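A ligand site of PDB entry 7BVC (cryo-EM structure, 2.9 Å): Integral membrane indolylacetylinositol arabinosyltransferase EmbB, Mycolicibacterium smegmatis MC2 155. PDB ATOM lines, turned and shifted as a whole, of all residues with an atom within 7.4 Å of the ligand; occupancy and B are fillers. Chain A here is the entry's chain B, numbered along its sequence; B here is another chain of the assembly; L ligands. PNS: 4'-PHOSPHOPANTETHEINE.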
ATOM      1  N   ARG A 250     -32.809 -10.291  27.115  1.00  0.00           N
ATOM      2  CA  ARG A 250     -31.443  -9.807  26.980  1.00  0.00           C
ATOM      3  C   ARG A 250     -30.481 -10.861  27.506  1.00  0.00           C
ATOM      4  O   ARG A 250     -30.860 -11.761  28.252  1.00  0.00           O
ATOM      5  CB  ARG A 250     -31.232  -8.490  27.728  1.00  0.00           C
ATOM      6  CG  ARG A 250     -32.422  -7.549  27.716  1.00  0.00           C
ATOM      7  CD  ARG A 250     -32.743  -7.069  26.312  1.00  0.00           C
ATOM      8  NE  ARG A 250     -33.574  -5.877  26.322  1.00  0.00           N
ATOM      9  CZ  ARG A 250     -34.325  -5.474  25.303  1.00  0.00           C
ATOM     10  NH1 ARG A 250     -34.351  -6.183  24.185  1.00  0.00           N
ATOM     11  NH2 ARG A 250     -35.043  -4.374  25.406  1.00  0.00           N
ATOM     12  N   MET A 251     -29.218 -10.740  27.096  1.00  0.00           N
ATOM     13  CA  MET A 251     -28.180 -11.605  27.624  1.00  0.00           C
ATOM     14  C   MET A 251     -27.839 -11.199  29.057  1.00  0.00           C
ATOM     15  O   MET A 251     -27.738 -10.014  29.374  1.00  0.00           O
ATOM     16  CB  MET A 251     -26.933 -11.565  26.746  1.00  0.00           C
ATOM     17  CG  MET A 251     -26.119 -10.279  26.834  1.00  0.00           C
ATOM     18  SD  MET A 251     -24.774 -10.209  25.638  1.00  0.00           S
ATOM     19  CE  MET A 251     -23.648 -11.423  26.312  1.00  0.00           C
ATOM     20  N   HIS A 252     -27.702 -12.194  29.928  1.00  0.00           N
ATOM     21  CA  HIS A 252     -27.347 -11.953  31.313  1.00  0.00           C
ATOM     22  C   HIS A 252     -25.864 -12.166  31.587  1.00  0.00           C
ATOM     23  O   HIS A 252     -25.391 -11.785  32.657  1.00  0.00           O
ATOM     24  CB  HIS A 252     -28.174 -12.844  32.242  1.00  0.00           C
ATOM     25  CG  HIS A 252     -29.573 -12.373  32.444  1.00  0.00           C
ATOM     26  ND1 HIS A 252     -29.903 -11.365  33.321  1.00  0.00           N
ATOM     27  CD2 HIS A 252     -30.740 -12.761  31.871  1.00  0.00           C
ATOM     28  CE1 HIS A 252     -31.206 -11.161  33.295  1.00  0.00           C
ATOM     29  NE2 HIS A 252     -31.740 -11.989  32.415  1.00  0.00           N
ATOM     30  N   ARG A 253     -25.140 -12.741  30.637  1.00  0.00           N
ATOM     31  CA  ARG A 253     -23.707 -12.990  30.768  1.00  0.00           C
ATOM     32  C   ARG A 253     -23.216 -13.544  29.443  1.00  0.00           C
ATOM     33  O   ARG A 253     -23.999 -13.896  28.552  1.00  0.00           O
ATOM     34  CB  ARG A 253     -23.398 -13.984  31.895  1.00  0.00           C
ATOM     35  CG  ARG A 253     -23.534 -15.434  31.490  1.00  0.00           C
ATOM     36  CD  ARG A 253     -23.734 -16.337  32.688  1.00  0.00           C
ATOM     37  NE  ARG A 253     -25.002 -16.052  33.358  1.00  0.00           N
ATOM     38  CZ  ARG A 253     -25.275 -16.385  34.611  1.00  0.00           C
ATOM     39  NH1 ARG A 253     -24.369 -17.015  35.336  1.00  0.00           N
ATOM     40  NH2 ARG A 253     -26.460 -16.095  35.130  1.00  0.00           N
ATOM     41  N   LEU A 254     -21.887 -13.603  29.314  1.00  0.00           N
ATOM     42  CA  LEU A 254     -21.241 -14.379  28.277  1.00  0.00           C
ATOM     43  C   LEU A 254     -20.636 -15.628  28.901  1.00  0.00           C
ATOM     44  O   LEU A 254     -20.502 -15.712  30.123  1.00  0.00           O
ATOM     45  CB  LEU A 254     -20.166 -13.564  27.544  1.00  0.00           C
ATOM     46  CG  LEU A 254     -18.861 -13.244  28.276  1.00  0.00           C
ATOM     47  CD1 LEU A 254     -17.808 -12.829  27.269  1.00  0.00           C
ATOM     48  CD2 LEU A 254     -19.059 -12.148  29.308  1.00  0.00           C
ATOM     49  N   ILE A 255     -20.267 -16.586  28.060  1.00  0.00           N
ATOM     50  CA  ILE A 255     -19.768 -17.882  28.518  1.00  0.00           C
ATOM     51  C   ILE A 255     -20.843 -18.523  29.396  1.00  0.00           C
ATOM     52  O   ILE A 255     -20.708 -18.528  30.628  1.00  0.00           O
ATOM     53  CB  ILE A 255     -18.434 -17.753  29.264  1.00  0.00           C
ATOM     54  CG1 ILE A 255     -17.437 -16.948  28.420  1.00  0.00           C
ATOM     55  CG2 ILE A 255     -17.853 -19.117  29.578  1.00  0.00           C
ATOM     56  CD1 ILE A 255     -17.291 -17.461  26.998  1.00  0.00           C
ATOM     57  N   PRO A 256     -21.948 -19.015  28.807  1.00  0.00           N
ATOM     58  CA  PRO A 256     -23.028 -19.619  29.606  1.00  0.00           C
ATOM     59  C   PRO A 256     -22.543 -20.686  30.575  1.00  0.00           C
ATOM     60  O   PRO A 256     -21.470 -21.272  30.375  1.00  0.00           O
ATOM     61  CB  PRO A 256     -23.965 -20.208  28.548  1.00  0.00           C
ATOM     62  CG  PRO A 256     -23.124 -20.342  27.317  1.00  0.00           C
ATOM     63  CD  PRO A 256     -22.178 -19.182  27.363  1.00  0.00           C
ATOM     64  N   THR A 257     -23.335 -20.957  31.617  1.00  0.00           N
ATOM     65  CA  THR A 257     -22.879 -21.794  32.719  1.00  0.00           C
ATOM     66  C   THR A 257     -22.616 -23.241  32.324  1.00  0.00           C
ATOM     67  O   THR A 257     -22.072 -23.991  33.134  1.00  0.00           O
ATOM     68  CB  THR A 257     -23.909 -21.765  33.852  1.00  0.00           C
ATOM     69  OG1 THR A 257     -25.055 -22.541  33.497  1.00  0.00           O
ATOM     70  CG2 THR A 257     -24.330 -20.334  34.148  1.00  0.00           C
ATOM     71  N   ARG A 258     -22.998 -23.663  31.124  1.00  0.00           N
ATOM     72  CA  ARG A 258     -22.662 -24.999  30.658  1.00  0.00           C
ATOM     73  C   ARG A 258     -21.340 -25.044  29.906  1.00  0.00           C
ATOM     74  O   ARG A 258     -20.892 -26.131  29.525  1.00  0.00           O
ATOM     75  CB  ARG A 258     -23.782 -25.569  29.775  1.00  0.00           C
ATOM     76  CG  ARG A 258     -23.722 -25.163  28.320  1.00  0.00           C
ATOM     77  CD  ARG A 258     -24.928 -25.704  27.573  1.00  0.00           C
ATOM     78  NE  ARG A 258     -24.931 -25.323  26.165  1.00  0.00           N
ATOM     79  CZ  ARG A 258     -25.936 -25.575  25.332  1.00  0.00           C
ATOM     80  NH1 ARG A 258     -27.020 -26.213  25.774  1.00  0.00           N
ATOM     81  NH2 ARG A 258     -25.864 -25.200  24.060  1.00  0.00           N
ATOM     82  N   TRP A 259     -20.697 -23.894  29.696  1.00  0.00           N
ATOM     83  CA  TRP A 259     -19.360 -23.875  29.112  1.00  0.00           C
ATOM     84  C   TRP A 259     -18.280 -24.090  30.173  1.00  0.00           C
ATOM     85  O   TRP A 259     -17.271 -24.727  29.906  1.00  0.00           O
ATOM     86  CB  TRP A 259     -19.124 -22.547  28.398  1.00  0.00           C
ATOM     87  CG  TRP A 259     -19.662 -22.484  27.016  1.00  0.00           C
ATOM     88  CD1 TRP A 259     -20.763 -23.125  26.541  1.00  0.00           C
ATOM     89  CD2 TRP A 259     -19.135 -21.717  25.929  1.00  0.00           C
ATOM     90  NE1 TRP A 259     -20.952 -22.818  25.215  1.00  0.00           N
ATOM     91  CE2 TRP A 259     -19.968 -21.955  24.818  1.00  0.00           C
ATOM     92  CE3 TRP A 259     -18.044 -20.869  25.786  1.00  0.00           C
ATOM     93  CZ2 TRP A 259     -19.734 -21.365  23.579  1.00  0.00           C
ATOM     94  CZ3 TRP A 259     -17.811 -20.282  24.560  1.00  0.00           C
ATOM     95  CH2 TRP A 259     -18.654 -20.532  23.467  1.00  0.00           C
ATOM     96  N   ARG A 260     -18.491 -23.544  31.378  1.00  0.00           N
ATOM     97  CA  ARG A 260     -17.480 -23.555  32.426  1.00  0.00           C
ATOM     98  C   ARG A 260     -17.418 -24.928  33.086  1.00  0.00           C
ATOM     99  O   ARG A 260     -17.855 -25.148  34.217  1.00  0.00           O
ATOM    100  CB  ARG A 260     -17.762 -22.457  33.435  1.00  0.00           C
ATOM    101  CG  ARG A 260     -19.225 -22.329  33.820  1.00  0.00           C
ATOM    102  CD  ARG A 260     -19.470 -21.082  34.654  1.00  0.00           C
ATOM    103  NE  ARG A 260     -19.282 -19.858  33.870  1.00  0.00           N
ATOM    104  CZ  ARG A 260     -19.908 -18.717  34.121  1.00  0.00           C
ATOM    105  NH1 ARG A 260     -20.766 -18.634  35.122  1.00  0.00           N
ATOM    106  NH2 ARG A 260     -19.674 -17.656  33.359  1.00  0.00           N
ATOM    107  N   LEU A 349     -14.043 -26.855  20.815  1.00  0.00           N
ATOM    108  CA  LEU A 349     -14.885 -26.075  21.725  1.00  0.00           C
ATOM    109  C   LEU A 349     -16.353 -26.193  21.354  1.00  0.00           C
ATOM    110  O   LEU A 349     -17.206 -26.509  22.206  1.00  0.00           O
ATOM    111  CB  LEU A 349     -14.445 -24.612  21.713  1.00  0.00           C
ATOM    112  CG  LEU A 349     -15.267 -23.631  22.543  1.00  0.00           C
ATOM    113  CD1 LEU A 349     -15.040 -23.865  24.033  1.00  0.00           C
ATOM    114  CD2 LEU A 349     -14.931 -22.202  22.165  1.00  0.00           C
ATOM    115  N   LEU A 350     -16.673 -25.947  20.082  1.00  0.00           N
ATOM    116  CA  LEU A 350     -18.070 -25.975  19.650  1.00  0.00           C
ATOM    117  C   LEU A 350     -18.655 -27.379  19.776  1.00  0.00           C
ATOM    118  O   LEU A 350     -19.736 -27.560  20.336  1.00  0.00           O
ATOM    119  CB  LEU A 350     -18.186 -25.465  18.214  1.00  0.00           C
ATOM    120  CG  LEU A 350     -17.934 -23.973  18.008  1.00  0.00           C
ATOM    121  CD1 LEU A 350     -18.205 -23.574  16.578  1.00  0.00           C
ATOM    122  CD2 LEU A 350     -18.776 -23.153  18.969  1.00  0.00           C
ATOM    123  N   GLU A 354     -21.616 -27.107  22.455  1.00  0.00           N
ATOM    124  CA  GLU A 354     -22.829 -26.622  21.814  1.00  0.00           C
ATOM    125  C   GLU A 354     -23.614 -27.736  21.119  1.00  0.00           C
ATOM    126  O   GLU A 354     -24.841 -27.685  21.104  1.00  0.00           O
ATOM    127  CB  GLU A 354     -22.486 -25.525  20.794  1.00  0.00           C
ATOM    128  CG  GLU A 354     -21.887 -24.274  21.406  1.00  0.00           C
ATOM    129  CD  GLU A 354     -22.879 -23.522  22.273  1.00  0.00           C
ATOM    130  OE1 GLU A 354     -24.076 -23.495  21.930  1.00  0.00           O
ATOM    131  OE2 GLU A 354     -22.463 -22.964  23.309  1.00  0.00           O
ATOM    132  N   ARG A 407     -29.036 -22.065  17.464  1.00  0.00           N
ATOM    133  CA  ARG A 407     -29.295 -20.958  18.376  1.00  0.00           C
ATOM    134  C   ARG A 407     -30.526 -20.159  17.952  1.00  0.00           C
ATOM    135  O   ARG A 407     -31.299 -19.711  18.798  1.00  0.00           O
ATOM    136  CB  ARG A 407     -28.072 -20.047  18.462  1.00  0.00           C
ATOM    137  CG  ARG A 407     -26.960 -20.574  19.337  1.00  0.00           C
ATOM    138  CD  ARG A 407     -27.376 -20.640  20.793  1.00  0.00           C
ATOM    139  NE  ARG A 407     -26.244 -20.911  21.660  1.00  0.00           N
ATOM    140  CZ  ARG A 407     -25.754 -20.037  22.537  1.00  0.00           C
ATOM    141  NH1 ARG A 407     -26.309 -18.846  22.676  1.00  0.00           N
ATOM    142  NH2 ARG A 407     -24.712 -20.366  23.288  1.00  0.00           N
ATOM    143  N   ASP B  40     -30.321 -27.507  31.328  1.00  0.00           N
ATOM    144  CA  ASP B  40     -29.667 -26.200  31.384  1.00  0.00           C
ATOM    145  C   ASP B  40     -30.660 -25.096  31.062  1.00  0.00           C
ATOM    146  O   ASP B  40     -31.725 -25.328  30.488  1.00  0.00           O
ATOM    147  CB  ASP B  40     -28.491 -26.155  30.419  1.00  0.00           C
ATOM    148  CG  ASP B  40     -28.799 -26.790  29.079  1.00  0.00           C
ATOM    149  OD1 ASP B  40     -29.887 -27.395  28.955  1.00  0.00           O
ATOM    150  OD2 ASP B  40     -27.976 -26.680  28.152  1.00  0.00           O
ATOM    151  N   SER B  41     -30.302 -23.865  31.443  1.00  0.00           N
ATOM    152  CA  SER B  41     -31.193 -22.739  31.215  1.00  0.00           C
ATOM    153  C   SER B  41     -31.322 -22.375  29.748  1.00  0.00           C
ATOM    154  O   SER B  41     -32.326 -21.759  29.358  1.00  0.00           O
ATOM    155  CB  SER B  41     -30.712 -21.528  32.011  1.00  0.00           C
ATOM    156  OG  SER B  41     -29.445 -21.130  31.558  1.00  0.00           O
ATOM    157  N   LEU B  42     -30.340 -22.722  28.914  1.00  0.00           N
ATOM    158  CA  LEU B  42     -30.492 -22.557  27.475  1.00  0.00           C
ATOM    159  C   LEU B  42     -31.604 -23.425  26.915  1.00  0.00           C
ATOM    160  O   LEU B  42     -32.023 -23.209  25.773  1.00  0.00           O
ATOM    161  CB  LEU B  42     -29.179 -22.847  26.765  1.00  0.00           C
ATOM    162  CG  LEU B  42     -28.371 -21.620  26.369  1.00  0.00           C
ATOM    163  CD1 LEU B  42     -27.025 -21.991  25.784  1.00  0.00           C
ATOM    164  CD2 LEU B  42     -29.163 -20.778  25.380  1.00  0.00           C
ATOM    165  N   SER B  43     -32.072 -24.412  27.671  1.00  0.00           N
ATOM    166  CA  SER B  43     -33.280 -25.157  27.338  1.00  0.00           C
ATOM    167  C   SER B  43     -34.510 -24.618  28.050  1.00  0.00           C
ATOM    168  O   SER B  43     -35.619 -24.754  27.528  1.00  0.00           O
ATOM    169  CB  SER B  43     -33.107 -26.638  27.696  1.00  0.00           C
ATOM    170  OG  SER B  43     -32.105 -27.242  26.905  1.00  0.00           O
ATOM    171  N   VAL B  45     -35.039 -21.464  28.314  1.00  0.00           N
ATOM    172  CA  VAL B  45     -35.457 -20.403  27.393  1.00  0.00           C
ATOM    173  C   VAL B  45     -36.302 -20.974  26.261  1.00  0.00           C
ATOM    174  O   VAL B  45     -37.317 -20.407  25.867  1.00  0.00           O
ATOM    175  CB  VAL B  45     -34.232 -19.646  26.866  1.00  0.00           C
ATOM    176  CG1 VAL B  45     -34.656 -18.559  25.877  1.00  0.00           C
ATOM    177  CG2 VAL B  45     -33.442 -19.043  28.014  1.00  0.00           C
ATOM    178  N   ASP B  61     -37.825 -13.060  31.610  1.00  0.00           N
ATOM    179  CA  ASP B  61     -36.587 -13.523  32.236  1.00  0.00           C
ATOM    180  C   ASP B  61     -36.380 -12.931  33.622  1.00  0.00           C
ATOM    181  O   ASP B  61     -35.500 -13.395  34.351  1.00  0.00           O
ATOM    182  CB  ASP B  61     -35.393 -13.187  31.342  1.00  0.00           C
ATOM    183  CG  ASP B  61     -35.385 -11.734  30.901  1.00  0.00           C
ATOM    184  OD1 ASP B  61     -36.403 -11.047  31.084  1.00  0.00           O
ATOM    185  OD2 ASP B  61     -34.349 -11.287  30.363  1.00  0.00           O
HETATM  186  O23 PNS L   1     -28.370 -19.224  32.739  1.00  0.00           O
HETATM  187  P24 PNS L   1     -27.185 -19.269  31.807  1.00  0.00           P
HETATM  188  O25 PNS L   1     -26.167 -18.238  32.225  1.00  0.00           O
HETATM  189  O26 PNS L   1     -26.563 -20.640  31.855  1.00  0.00           O
HETATM  190  O27 PNS L   1     -27.694 -18.969  30.267  1.00  0.00           O
HETATM  191  C28 PNS L   1     -28.839 -18.200  30.085  1.00  0.00           C
HETATM  192  C29 PNS L   1     -28.584 -17.179  28.982  1.00  0.00           C
HETATM  193  C30 PNS L   1     -28.814 -17.828  27.625  1.00  0.00           C
HETATM  194  C31 PNS L   1     -29.567 -16.022  29.165  1.00  0.00           C
HETATM  195  C32 PNS L   1     -27.137 -16.694  29.087  1.00  0.00           C
HETATM  196  O33 PNS L   1     -26.296 -17.809  29.145  1.00  0.00           O
HETATM  197  C34 PNS L   1     -26.723 -15.878  27.869  1.00  0.00           C
HETATM  198  O35 PNS L   1     -27.165 -14.790  27.678  1.00  0.00           O
HETATM  199  N36 PNS L   1     -25.748 -16.420  26.943  1.00  0.00           N
HETATM  200  C37 PNS L   1     -25.352 -15.648  25.794  1.00  0.00           C
HETATM  201  C38 PNS L   1     -23.889 -15.933  25.470  1.00  0.00           C
HETATM  202  C39 PNS L   1     -23.617 -16.935  24.350  1.00  0.00           C
HETATM  203  O40 PNS L   1     -24.492 -17.610  23.941  1.00  0.00           O
HETATM  204  N41 PNS L   1     -22.290 -17.053  23.787  1.00  0.00           N
HETATM  205  C42 PNS L   1     -21.205 -16.219  24.278  1.00  0.00           C
HETATM  206  C43 PNS L   1     -20.169 -16.039  23.176  1.00  0.00           C
HETATM  207  S44 PNS L   1     -20.131 -17.548  22.173  1.00  0.00           S
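The guanidinium group (NE) of Arg 407 lies within salt-bridge range of the side-chain carboxylate (OE1) of Glu 354, at 3.4 Å.
OD2 of Asp 61 of chain B sits at hydrogen-bond distance from NE2 of His 252 (3.4 Å).
The side-chain carboxylate (OE2) of Glu 354 lies within hydrogen-bond range of the indole nitrogen (NE1) of Trp 259 (2.4 Å).
NH2 of Arg 260 lies within hydrogen-bond range of O of Ile 255, 3.0 Å away.
Merely in contact with the ligand: Met 251, Ile 255, Pro 256, Trp 259 and Leu 42 of chain B.
Of the 21 residues printed, 10 come within 4 Å of the ligand.
The nearest printed residue that does not touch the ligand is Leu 254 (4.2 Å).
O23 of the ligand sits at hydrogen-bond distance from OG of Ser 41 of chain B.
An oxygen (O40) of the ligand sits at hydrogen-bond distance from the guanidinium group of Arg 407 (2.5 Å).
The backbone carbonyl oxygen (O) of Arg 253 lies close to a nitrogen (N36) of the ligand, at 3.5 Å.
The guanidinium group (NE) of Arg 253 lies within salt-bridge range of an oxygen (O25) of the ligand, at 2.7 Å.
O26 of the ligand lies close to N of Thr 257.
An oxygen (O26) of the ligand lies within hydrogen-bond range of the side-chain hydroxyl (OG1) of Thr 257 (2.9 Å).
The backbone NH of His 252 lies within hydrogen-bond range of an oxygen (O35) of the ligand (3.5 Å).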
